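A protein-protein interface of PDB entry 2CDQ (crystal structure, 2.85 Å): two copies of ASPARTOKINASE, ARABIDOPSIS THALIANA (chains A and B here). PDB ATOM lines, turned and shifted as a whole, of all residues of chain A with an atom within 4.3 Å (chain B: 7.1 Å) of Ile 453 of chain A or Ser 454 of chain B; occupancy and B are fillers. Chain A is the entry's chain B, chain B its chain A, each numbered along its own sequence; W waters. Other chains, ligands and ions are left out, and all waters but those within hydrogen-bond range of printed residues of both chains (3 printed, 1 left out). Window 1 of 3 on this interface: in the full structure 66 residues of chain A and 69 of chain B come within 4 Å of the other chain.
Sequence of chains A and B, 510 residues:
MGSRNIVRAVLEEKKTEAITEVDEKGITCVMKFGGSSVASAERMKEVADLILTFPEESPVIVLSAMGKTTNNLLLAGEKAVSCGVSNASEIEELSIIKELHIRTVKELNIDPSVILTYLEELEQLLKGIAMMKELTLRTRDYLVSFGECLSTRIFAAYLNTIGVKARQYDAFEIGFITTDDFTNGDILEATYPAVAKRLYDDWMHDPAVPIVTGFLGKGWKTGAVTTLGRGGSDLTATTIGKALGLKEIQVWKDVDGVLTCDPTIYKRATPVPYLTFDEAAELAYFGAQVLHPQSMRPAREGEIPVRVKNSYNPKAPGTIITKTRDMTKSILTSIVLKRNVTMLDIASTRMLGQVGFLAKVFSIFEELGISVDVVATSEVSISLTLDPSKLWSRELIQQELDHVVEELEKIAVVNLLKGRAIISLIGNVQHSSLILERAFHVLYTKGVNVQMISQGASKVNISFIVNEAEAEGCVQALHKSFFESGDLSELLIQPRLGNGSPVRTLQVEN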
ATOM      1  N   ALA A 376      10.551  25.122 -16.238  1.00  0.00           N
ATOM      2  CA  ALA A 376      11.191  24.985 -17.551  1.00  0.00           C
ATOM      3  C   ALA A 376      10.277  24.190 -18.472  1.00  0.00           C
ATOM      4  O   ALA A 376       9.325  23.566 -18.001  1.00  0.00           O
ATOM      5  CB  ALA A 376      12.543  24.300 -17.423  1.00  0.00           C
ATOM      6  N   THR A 377      10.555  24.211 -19.774  1.00  0.00           N
ATOM      7  CA  THR A 377       9.687  23.552 -20.748  1.00  0.00           C
ATOM      8  C   THR A 377      10.454  22.777 -21.800  1.00  0.00           C
ATOM      9  O   THR A 377      11.658  22.963 -21.964  1.00  0.00           O
ATOM     10  CB  THR A 377       8.803  24.569 -21.491  1.00  0.00           C
ATOM     11  OG1 THR A 377       9.609  25.664 -21.949  1.00  0.00           O
ATOM     12  CG2 THR A 377       7.671  25.083 -20.592  1.00  0.00           C
ATOM     13  N   PHE A 440      29.703  24.390 -16.496  1.00  0.00           N
ATOM     14  CA  PHE A 440      29.453  23.044 -16.992  1.00  0.00           C
ATOM     15  C   PHE A 440      30.731  22.242 -17.142  1.00  0.00           C
ATOM     16  O   PHE A 440      30.710  21.015 -17.017  1.00  0.00           O
ATOM     17  CB  PHE A 440      28.646  23.067 -18.287  1.00  0.00           C
ATOM     18  CG  PHE A 440      27.202  23.378 -18.071  1.00  0.00           C
ATOM     19  CD1 PHE A 440      26.712  24.659 -18.300  1.00  0.00           C
ATOM     20  CD2 PHE A 440      26.331  22.395 -17.599  1.00  0.00           C
ATOM     21  CE1 PHE A 440      25.373  24.956 -18.082  1.00  0.00           C
ATOM     22  CE2 PHE A 440      24.987  22.677 -17.376  1.00  0.00           C
ATOM     23  CZ  PHE A 440      24.506  23.959 -17.617  1.00  0.00           C
ATOM     24  N   VAL A 450      23.298  18.145 -15.009  1.00  0.00           N
ATOM     25  CA  VAL A 450      22.168  18.925 -14.524  1.00  0.00           C
ATOM     26  C   VAL A 450      20.875  18.344 -15.084  1.00  0.00           C
ATOM     27  O   VAL A 450      20.773  18.055 -16.274  1.00  0.00           O
ATOM     28  CB  VAL A 450      22.322  20.415 -14.913  1.00  0.00           C
ATOM     29  CG1 VAL A 450      21.058  21.185 -14.620  1.00  0.00           C
ATOM     30  CG2 VAL A 450      23.501  21.034 -14.174  1.00  0.00           C
ATOM     31  N   MET A 452      17.771  19.844 -14.871  1.00  0.00           N
ATOM     32  CA  MET A 452      16.850  20.887 -15.343  1.00  0.00           C
ATOM     33  C   MET A 452      17.481  22.274 -15.225  1.00  0.00           C
ATOM     34  O   MET A 452      18.060  22.605 -14.184  1.00  0.00           O
ATOM     35  CB  MET A 452      15.524  20.794 -14.573  1.00  0.00           C
ATOM     36  CG  MET A 452      14.616  22.006 -14.627  1.00  0.00           C
ATOM     37  SD  MET A 452      13.061  21.645 -13.778  1.00  0.00           S
ATOM     38  CE  MET A 452      12.277  23.257 -13.808  1.00  0.00           C
ATOM     39  N   ILE A 453      17.381  23.069 -16.294  1.00  0.00           N
ATOM     40  CA  ILE A 453      18.005  24.400 -16.348  1.00  0.00           C
ATOM     41  C   ILE A 453      16.961  25.466 -16.668  1.00  0.00           C
ATOM     42  O   ILE A 453      16.142  25.278 -17.564  1.00  0.00           O
ATOM     43  CB  ILE A 453      19.157  24.472 -17.403  1.00  0.00           C
ATOM     44  CG1 ILE A 453      20.060  23.235 -17.336  1.00  0.00           C
ATOM     45  CG2 ILE A 453      19.990  25.741 -17.223  1.00  0.00           C
ATOM     46  CD1 ILE A 453      20.829  22.959 -18.611  1.00  0.00           C
ATOM     47  N   SER A 454      16.996  26.583 -15.939  1.00  0.00           N
ATOM     48  CA  SER A 454      16.036  27.671 -16.144  1.00  0.00           C
ATOM     49  C   SER A 454      16.619  29.067 -15.884  1.00  0.00           C
ATOM     50  O   SER A 454      16.933  29.414 -14.747  1.00  0.00           O
ATOM     51  CB  SER A 454      14.782  27.437 -15.289  1.00  0.00           C
ATOM     52  OG  SER A 454      13.864  28.520 -15.377  1.00  0.00           O
ATOM     53  N   ILE A 462      20.646  31.968 -12.784  1.00  0.00           N
ATOM     54  CA  ILE A 462      20.407  30.751 -13.570  1.00  0.00           C
ATOM     55  C   ILE A 462      20.419  29.522 -12.667  1.00  0.00           C
ATOM     56  O   ILE A 462      21.360  29.319 -11.897  1.00  0.00           O
ATOM     57  CB  ILE A 462      21.398  30.598 -14.762  1.00  0.00           C
ATOM     58  CG1 ILE A 462      21.167  29.271 -15.489  1.00  0.00           C
ATOM     59  CG2 ILE A 462      22.848  30.741 -14.303  1.00  0.00           C
ATOM     60  CD1 ILE A 462      22.167  28.980 -16.576  1.00  0.00           C
ATOM     61  N   SER A 463      19.372  28.707 -12.766  1.00  0.00           N
ATOM     62  CA  SER A 463      19.193  27.571 -11.861  1.00  0.00           C
ATOM     63  C   SER A 463      19.483  26.223 -12.502  1.00  0.00           C
ATOM     64  O   SER A 463      19.050  25.949 -13.619  1.00  0.00           O
ATOM     65  CB  SER A 463      17.778  27.574 -11.283  1.00  0.00           C
ATOM     66  OG  SER A 463      17.548  28.753 -10.530  1.00  0.00           O
ATOM     67  N   PHE A 464      20.230  25.393 -11.780  1.00  0.00           N
ATOM     68  CA  PHE A 464      20.445  24.005 -12.161  1.00  0.00           C
ATOM     69  C   PHE A 464      19.774  23.111 -11.152  1.00  0.00           C
ATOM     70  O   PHE A 464      20.013  23.248  -9.953  1.00  0.00           O
ATOM     71  CB  PHE A 464      21.928  23.641 -12.128  1.00  0.00           C
ATOM     72  CG  PHE A 464      22.809  24.551 -12.911  1.00  0.00           C
ATOM     73  CD1 PHE A 464      24.027  24.955 -12.382  1.00  0.00           C
ATOM     74  CD2 PHE A 464      22.439  24.993 -14.178  1.00  0.00           C
ATOM     75  CE1 PHE A 464      24.866  25.793 -13.097  1.00  0.00           C
ATOM     76  CE2 PHE A 464      23.269  25.832 -14.903  1.00  0.00           C
ATOM     77  CZ  PHE A 464      24.485  26.235 -14.363  1.00  0.00           C
ATOM     78  N   VAL B 374       8.147  28.485 -25.036  1.00  0.00           N
ATOM     79  CA  VAL B 374       9.216  28.236 -24.068  1.00  0.00           C
ATOM     80  C   VAL B 374       8.971  29.049 -22.787  1.00  0.00           C
ATOM     81  O   VAL B 374       8.491  30.183 -22.857  1.00  0.00           O
ATOM     82  CB  VAL B 374      10.593  28.571 -24.698  1.00  0.00           C
ATOM     83  CG1 VAL B 374      11.727  28.373 -23.715  1.00  0.00           C
ATOM     84  CG2 VAL B 374      10.811  27.728 -25.936  1.00  0.00           C
ATOM     85  N   VAL B 375       9.271  28.460 -21.628  1.00  0.00           N
ATOM     86  CA  VAL B 375       9.082  29.138 -20.335  1.00  0.00           C
ATOM     87  C   VAL B 375      10.296  28.928 -19.425  1.00  0.00           C
ATOM     88  O   VAL B 375      10.875  27.836 -19.377  1.00  0.00           O
ATOM     89  CB  VAL B 375       7.779  28.683 -19.598  1.00  0.00           C
ATOM     90  CG1 VAL B 375       7.709  29.250 -18.185  1.00  0.00           C
ATOM     91  CG2 VAL B 375       6.535  29.094 -20.365  1.00  0.00           C
ATOM     92  N   ALA B 376      10.676  29.993 -18.722  1.00  0.00           N
ATOM     93  CA  ALA B 376      11.702  29.942 -17.686  1.00  0.00           C
ATOM     94  C   ALA B 376      11.323  30.898 -16.564  1.00  0.00           C
ATOM     95  O   ALA B 376      10.390  31.690 -16.712  1.00  0.00           O
ATOM     96  CB  ALA B 376      13.063  30.297 -18.257  1.00  0.00           C
ATOM     97  N   THR B 377      12.043  30.827 -15.448  1.00  0.00           N
ATOM     98  CA  THR B 377      11.715  31.632 -14.274  1.00  0.00           C
ATOM     99  C   THR B 377      12.957  32.161 -13.585  1.00  0.00           C
ATOM    100  O   THR B 377      14.062  31.682 -13.834  1.00  0.00           O
ATOM    101  CB  THR B 377      10.959  30.800 -13.232  1.00  0.00           C
ATOM    102  OG1 THR B 377      11.645  29.561 -13.038  1.00  0.00           O
ATOM    103  CG2 THR B 377       9.526  30.527 -13.681  1.00  0.00           C
ATOM    104  N   SER B 424      17.512  25.277 -30.454  1.00  0.00           N
ATOM    105  CA  SER B 424      17.290  24.093 -29.634  1.00  0.00           C
ATOM    106  C   SER B 424      18.385  23.070 -29.885  1.00  0.00           C
ATOM    107  O   SER B 424      18.645  22.701 -31.029  1.00  0.00           O
ATOM    108  CB  SER B 424      15.918  23.477 -29.914  1.00  0.00           C
ATOM    109  OG  SER B 424      14.902  24.103 -29.149  1.00  0.00           O
ATOM    110  N   SER B 432      25.039  15.816 -21.118  1.00  0.00           N
ATOM    111  CA  SER B 432      24.525  17.167 -20.974  1.00  0.00           C
ATOM    112  C   SER B 432      25.626  18.199 -20.701  1.00  0.00           C
ATOM    113  O   SER B 432      25.786  19.153 -21.466  1.00  0.00           O
ATOM    114  CB  SER B 432      23.472  17.205 -19.867  1.00  0.00           C
ATOM    115  OG  SER B 432      23.059  18.537 -19.615  1.00  0.00           O
ATOM    116  N   LEU B 436      27.065  21.092 -23.066  1.00  0.00           N
ATOM    117  CA  LEU B 436      26.870  22.473 -22.640  1.00  0.00           C
ATOM    118  C   LEU B 436      28.154  23.267 -22.507  1.00  0.00           C
ATOM    119  O   LEU B 436      28.183  24.442 -22.872  1.00  0.00           O
ATOM    120  CB  LEU B 436      26.030  22.547 -21.361  1.00  0.00           C
ATOM    121  CG  LEU B 436      24.524  22.795 -21.528  1.00  0.00           C
ATOM    122  CD1 LEU B 436      24.067  22.758 -22.979  1.00  0.00           C
ATOM    123  CD2 LEU B 436      23.722  21.813 -20.703  1.00  0.00           C
ATOM    124  N   PHE B 440      28.448  26.601 -25.037  1.00  0.00           N
ATOM    125  CA  PHE B 440      28.730  27.922 -24.495  1.00  0.00           C
ATOM    126  C   PHE B 440      30.141  28.396 -24.800  1.00  0.00           C
ATOM    127  O   PHE B 440      30.369  29.604 -24.933  1.00  0.00           O
ATOM    128  CB  PHE B 440      28.426  27.980 -23.004  1.00  0.00           C
ATOM    129  CG  PHE B 440      26.961  27.981 -22.705  1.00  0.00           C
ATOM    130  CD1 PHE B 440      26.313  26.806 -22.333  1.00  0.00           C
ATOM    131  CD2 PHE B 440      26.217  29.153 -22.830  1.00  0.00           C
ATOM    132  CE1 PHE B 440      24.952  26.804 -22.073  1.00  0.00           C
ATOM    133  CE2 PHE B 440      24.856  29.160 -22.568  1.00  0.00           C
ATOM    134  CZ  PHE B 440      24.219  27.988 -22.191  1.00  0.00           C
ATOM    135  N   VAL B 450      23.355  34.190 -24.439  1.00  0.00           N
ATOM    136  CA  VAL B 450      22.006  33.655 -24.487  1.00  0.00           C
ATOM    137  C   VAL B 450      21.139  34.424 -23.506  1.00  0.00           C
ATOM    138  O   VAL B 450      21.502  34.579 -22.338  1.00  0.00           O
ATOM    139  CB  VAL B 450      22.001  32.148 -24.150  1.00  0.00           C
ATOM    140  CG1 VAL B 450      20.587  31.633 -23.986  1.00  0.00           C
ATOM    141  CG2 VAL B 450      22.735  31.363 -25.234  1.00  0.00           C
ATOM    142  N   MET B 452      17.900  33.660 -22.626  1.00  0.00           N
ATOM    143  CA  MET B 452      16.987  32.811 -21.873  1.00  0.00           C
ATOM    144  C   MET B 452      17.339  31.348 -22.123  1.00  0.00           C
ATOM    145  O   MET B 452      17.530  30.944 -23.273  1.00  0.00           O
ATOM    146  CB  MET B 452      15.542  33.118 -22.292  1.00  0.00           C
ATOM    147  CG  MET B 452      14.458  32.265 -21.664  1.00  0.00           C
ATOM    148  SD  MET B 452      12.819  32.923 -22.063  1.00  0.00           S
ATOM    149  CE  MET B 452      11.779  31.544 -21.603  1.00  0.00           C
ATOM    150  N   ILE B 453      17.448  30.566 -21.048  1.00  0.00           N
ATOM    151  CA  ILE B 453      17.763  29.136 -21.152  1.00  0.00           C
ATOM    152  C   ILE B 453      16.634  28.316 -20.520  1.00  0.00           C
ATOM    153  O   ILE B 453      16.080  28.710 -19.489  1.00  0.00           O
ATOM    154  CB  ILE B 453      19.139  28.783 -20.502  1.00  0.00           C
ATOM    155  CG1 ILE B 453      20.225  29.774 -20.934  1.00  0.00           C
ATOM    156  CG2 ILE B 453      19.576  27.363 -20.871  1.00  0.00           C
ATOM    157  CD1 ILE B 453      21.425  29.840 -20.011  1.00  0.00           C
ATOM    158  N   SER B 454      16.281  27.191 -21.145  1.00  0.00           N
ATOM    159  CA  SER B 454      15.205  26.343 -20.629  1.00  0.00           C
ATOM    160  C   SER B 454      15.345  24.865 -20.995  1.00  0.00           C
ATOM    161  O   SER B 454      15.217  24.485 -22.162  1.00  0.00           O
ATOM    162  CB  SER B 454      13.837  26.883 -21.066  1.00  0.00           C
ATOM    163  OG  SER B 454      12.775  26.116 -20.525  1.00  0.00           O
ATOM    164  N   GLN B 455      15.615  24.044 -19.982  1.00  0.00           N
ATOM    165  CA  GLN B 455      15.642  22.589 -20.125  1.00  0.00           C
ATOM    166  C   GLN B 455      14.792  21.943 -19.044  1.00  0.00           C
ATOM    167  O   GLN B 455      14.950  22.244 -17.863  1.00  0.00           O
ATOM    168  CB  GLN B 455      17.070  22.050 -20.042  1.00  0.00           C
ATOM    169  CG  GLN B 455      17.154  20.525 -20.047  1.00  0.00           C
ATOM    170  CD  GLN B 455      18.575  20.016 -19.956  1.00  0.00           C
ATOM    171  OE1 GLN B 455      19.392  20.248 -20.847  1.00  0.00           O
ATOM    172  NE2 GLN B 455      18.878  19.305 -18.878  1.00  0.00           N
ATOM    173  N   GLY B 456      13.896  21.050 -19.452  1.00  0.00           N
ATOM    174  CA  GLY B 456      13.019  20.343 -18.518  1.00  0.00           C
ATOM    175  C   GLY B 456      13.653  19.073 -17.998  1.00  0.00           C
ATOM    176  O   GLY B 456      14.743  18.706 -18.430  1.00  0.00           O
ATOM    177  N   ALA B 457      12.954  18.404 -17.081  1.00  0.00           N
ATOM    178  CA  ALA B 457      13.461  17.225 -16.358  1.00  0.00           C
ATOM    179  C   ALA B 457      14.108  16.169 -17.254  1.00  0.00           C
ATOM    180  O   ALA B 457      13.412  15.389 -17.902  1.00  0.00           O
ATOM    181  CB  ALA B 457      12.352  16.605 -15.529  1.00  0.00           C
ATOM    182  N   ASN B 461      15.993  17.999 -25.056  1.00  0.00           N
ATOM    183  CA  ASN B 461      15.860  19.316 -25.682  1.00  0.00           C
ATOM    184  C   ASN B 461      16.222  20.453 -24.725  1.00  0.00           C
ATOM    185  O   ASN B 461      15.573  20.635 -23.695  1.00  0.00           O
ATOM    186  CB  ASN B 461      14.408  19.480 -26.173  1.00  0.00           C
ATOM    187  CG  ASN B 461      14.142  20.815 -26.875  1.00  0.00           C
ATOM    188  OD1 ASN B 461      14.769  21.835 -26.590  1.00  0.00           O
ATOM    189  ND2 ASN B 461      13.180  20.808 -27.789  1.00  0.00           N
ATOM    190  N   ILE B 462      17.251  21.221 -25.069  1.00  0.00           N
ATOM    191  CA  ILE B 462      17.560  22.453 -24.336  1.00  0.00           C
ATOM    192  C   ILE B 462      17.521  23.664 -25.266  1.00  0.00           C
ATOM    193  O   ILE B 462      18.117  23.647 -26.343  1.00  0.00           O
ATOM    194  CB  ILE B 462      18.904  22.366 -23.565  1.00  0.00           C
ATOM    195  CG1 ILE B 462      19.170  23.663 -22.795  1.00  0.00           C
ATOM    196  CG2 ILE B 462      20.060  22.013 -24.498  1.00  0.00           C
ATOM    197  CD1 ILE B 462      20.553  23.746 -22.171  1.00  0.00           C
ATOM    198  N   SER B 463      16.807  24.706 -24.849  1.00  0.00           N
ATOM    199  CA  SER B 463      16.594  25.871 -25.699  1.00  0.00           C
ATOM    200  C   SER B 463      17.349  27.115 -25.229  1.00  0.00           C
ATOM    201  O   SER B 463      17.358  27.428 -24.038  1.00  0.00           O
ATOM    202  CB  SER B 463      15.098  26.171 -25.814  1.00  0.00           C
ATOM    203  OG  SER B 463      14.407  25.078 -26.397  1.00  0.00           O
ATOM    204  N   PHE B 464      17.986  27.803 -26.176  1.00  0.00           N
ATOM    205  CA  PHE B 464      18.555  29.131 -25.941  1.00  0.00           C
ATOM    206  C   PHE B 464      17.754  30.168 -26.696  1.00  0.00           C
ATOM    207  O   PHE B 464      17.451  29.983 -27.877  1.00  0.00           O
ATOM    208  CB  PHE B 464      19.988  29.251 -26.465  1.00  0.00           C
ATOM    209  CG  PHE B 464      20.894  28.137 -26.068  1.00  0.00           C
ATOM    210  CD1 PHE B 464      21.775  27.603 -26.999  1.00  0.00           C
ATOM    211  CD2 PHE B 464      20.885  27.629 -24.774  1.00  0.00           C
ATOM    212  CE1 PHE B 464      22.632  26.575 -26.652  1.00  0.00           C
ATOM    213  CE2 PHE B 464      21.736  26.596 -24.414  1.00  0.00           C
ATOM    214  CZ  PHE B 464      22.612  26.066 -25.354  1.00  0.00           C
ATOM    215  N   ILE B 465      17.443  31.273 -26.034  1.00  0.00           N
ATOM    216  CA  ILE B 465      16.882  32.426 -26.738  1.00  0.00           C
ATOM    217  C   ILE B 465      17.998  33.401 -27.120  1.00  0.00           C
ATOM    218  O   ILE B 465      18.784  33.852 -26.282  1.00  0.00           O
ATOM    219  CB  ILE B 465      15.731  33.102 -25.963  1.00  0.00           C
ATOM    220  CG1 ILE B 465      14.447  32.291 -26.128  1.00  0.00           C
ATOM    221  CG2 ILE B 465      15.504  34.529 -26.446  1.00  0.00           C
ATOM    222  CD1 ILE B 465      14.429  30.984 -25.360  1.00  0.00           C
HETATM  223  O   HOH W   1      13.433  21.016 -22.098  1.00  0.00           O
HETATM  224  O   HOH W   2      24.610  19.160 -17.108  1.00  0.00           O
HETATM  225  O   HOH W   3      16.362  30.438 -12.296  1.00  0.00           O
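The backbone carbonyl oxygen of Val 375 of chain B is in hydrogen-bond range of the side-chain hydroxyl of Ser 454 of chain B (2.8 Å).
The backbone NH (N) of Ser 454 of chain B sits at hydrogen-bond distance from the backbone carbonyl oxygen (O) of Ser 463 of chain B (3.1 Å).
N of Ser 454 of chain A is in hydrogen-bond range of O of Ser 463 of chain A (3.2 Å).
Ala 376 of chain A touches Val 375 of chain B (CA to O, 3.4 Å).
Ala 376 of chain A touches Ser 454 of chain B.
Ala 376 of chain A touches Gln 455 of chain B (CB to O, 3.2 Å).
Val 374 of chain B touches Thr 377 of chain A.
Thr 377 of chain A touches Gly 456 of chain B.
Leu 436 of chain B touches Phe 440 of chain A.
Ile 453 of chain A touches Leu 436 of chain B (CD1 to CD2, 3.7 Å).
Ile 453 of chain A touches Ile 453 of chain B (O to O, 3.9 Å).
Ser 454 of chain A touches Ala 376 of chain B.
Ser 454 of chain A touches Ile 453 of chain B.
Of the 20 printed residues of chain B, 10 touch a printed residue of chain A.
Printed residues of chain B that touch a printed residue of chain A: Val 374, Val 375, Ala 376, Thr 377, Leu 436, Ile 453, Ser 454, Gln 455, Gly 456 and Ile 462.
Hydrophobic or aromatic side chains of chain B that line the printed part of chain A: Val 374, Val 375, Ala 376, Leu 436, Ile 453 and Ile 462.
Of the 10 printed residues of chain A, 8 touch a printed residue of chain B.
Hydrophobic or aromatic side chains of chain A within 4 Å of the printed part of chain B: Ala 376, Phe 440, Met 452, Ile 453 and Ile 462.
Among the printed residues, no Asp or Glu carboxylate lies within 4 Å of a Lys or Arg side-chain nitrogen of the other chain.
Water W1 lies within hydrogen-bond range of the backbone carbonyl oxygen (O) of Thr 377 of chain A (2.6 Å), the backbone NH (N) of Gly 456 of chain B (2.7 Å) and the backbone carbonyl oxygen (O) of Asn 461 of chain B (2.7 Å).
Water W2 lies within hydrogen-bond range of the backbone NH of Val 450 of chain A (2.7 Å) and the side-chain hydroxyl of Ser 432 of chain B (3.0 Å).
Water W3 lies within hydrogen-bond range of the side-chain hydroxyl of Ser 463 of chain A (2.7 Å), the backbone carbonyl oxygen of Ser 454 of chain A (2.7 Å) and the backbone carbonyl oxygen of Thr 377 of chain B (3.0 Å).
N of Val 375 of chain B is in hydrogen-bond range of OG1 of Thr 377 of chain A.
The side-chain hydroxyl of Ser 454 of chain A lies within hydrogen-bond range of the backbone NH of Thr 377 of chain B, 2.9 Å away.
The side-chain hydroxyl (OG) of Ser 454 of chain B lies within hydrogen-bond range of the backbone NH (N) of Thr 377 of chain A (3.0 Å).
The side-chain amide nitrogen of Gln 455 of chain B is in hydrogen-bond range of the backbone carbonyl oxygen of Val 450 of chain A, at 3.5 Å.
The backbone NH of Gln 455 of chain B lies within hydrogen-bond range of the backbone carbonyl oxygen of Ile 453 of chain A, at 2.8 Å.
Ala 376 of chain A touches Ser 454 of chain B, and with the chains exchanged Ser 454 of chain A touches Ala 376 of chain B.
Thr 377 of chain A touches Ser 454 of chain B, and with the chains exchanged Ser 454 of chain A touches Thr 377 of chain B.
Ile 453 of chain B touches its own counterpart, Ile 453 of chain A.
Ile 453 of chain A touches Ser 454 of chain B, and with the chains exchanged Ser 454 of chain A touches Ile 453 of chain B.
Of the 19 pairs that touch across the chains among the printed residues, 9 have their exchanged pair printed and touching as well.
Of the printed residues of chain B, Phe 440 of chain A touches Leu 436.
Of the printed residues of chain B, Ile 453 of chain A touches Leu 436, Ile 453, Ser 454, Gln 455 and Ile 462.
Val 450 of chain B touches none of the printed residues of chain A.
Printed residues of chain A within 4 Å of Ile 453 of chain B: Ile 453, Ser 454 and Ile 462.
Ser 454 of chain B touches just these residues of chain A: Ala 376 (3.6 Å), Thr 377 (3.0 Å) and Ile 453 (3.4 Å).
Of the printed residues of chain A, Gln 455 of chain B touches Ala 376, Val 450, Met 452 and Ile 453.
Of the printed residues of chain A, Gly 456 of chain B touches Thr 377.
Ser 463 of chain B touches none of the printed residues of chain A.
The nearest residue of chain B that does not touch Ile 453 of chain A is Ser 432 of chain B (5.1 Å).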
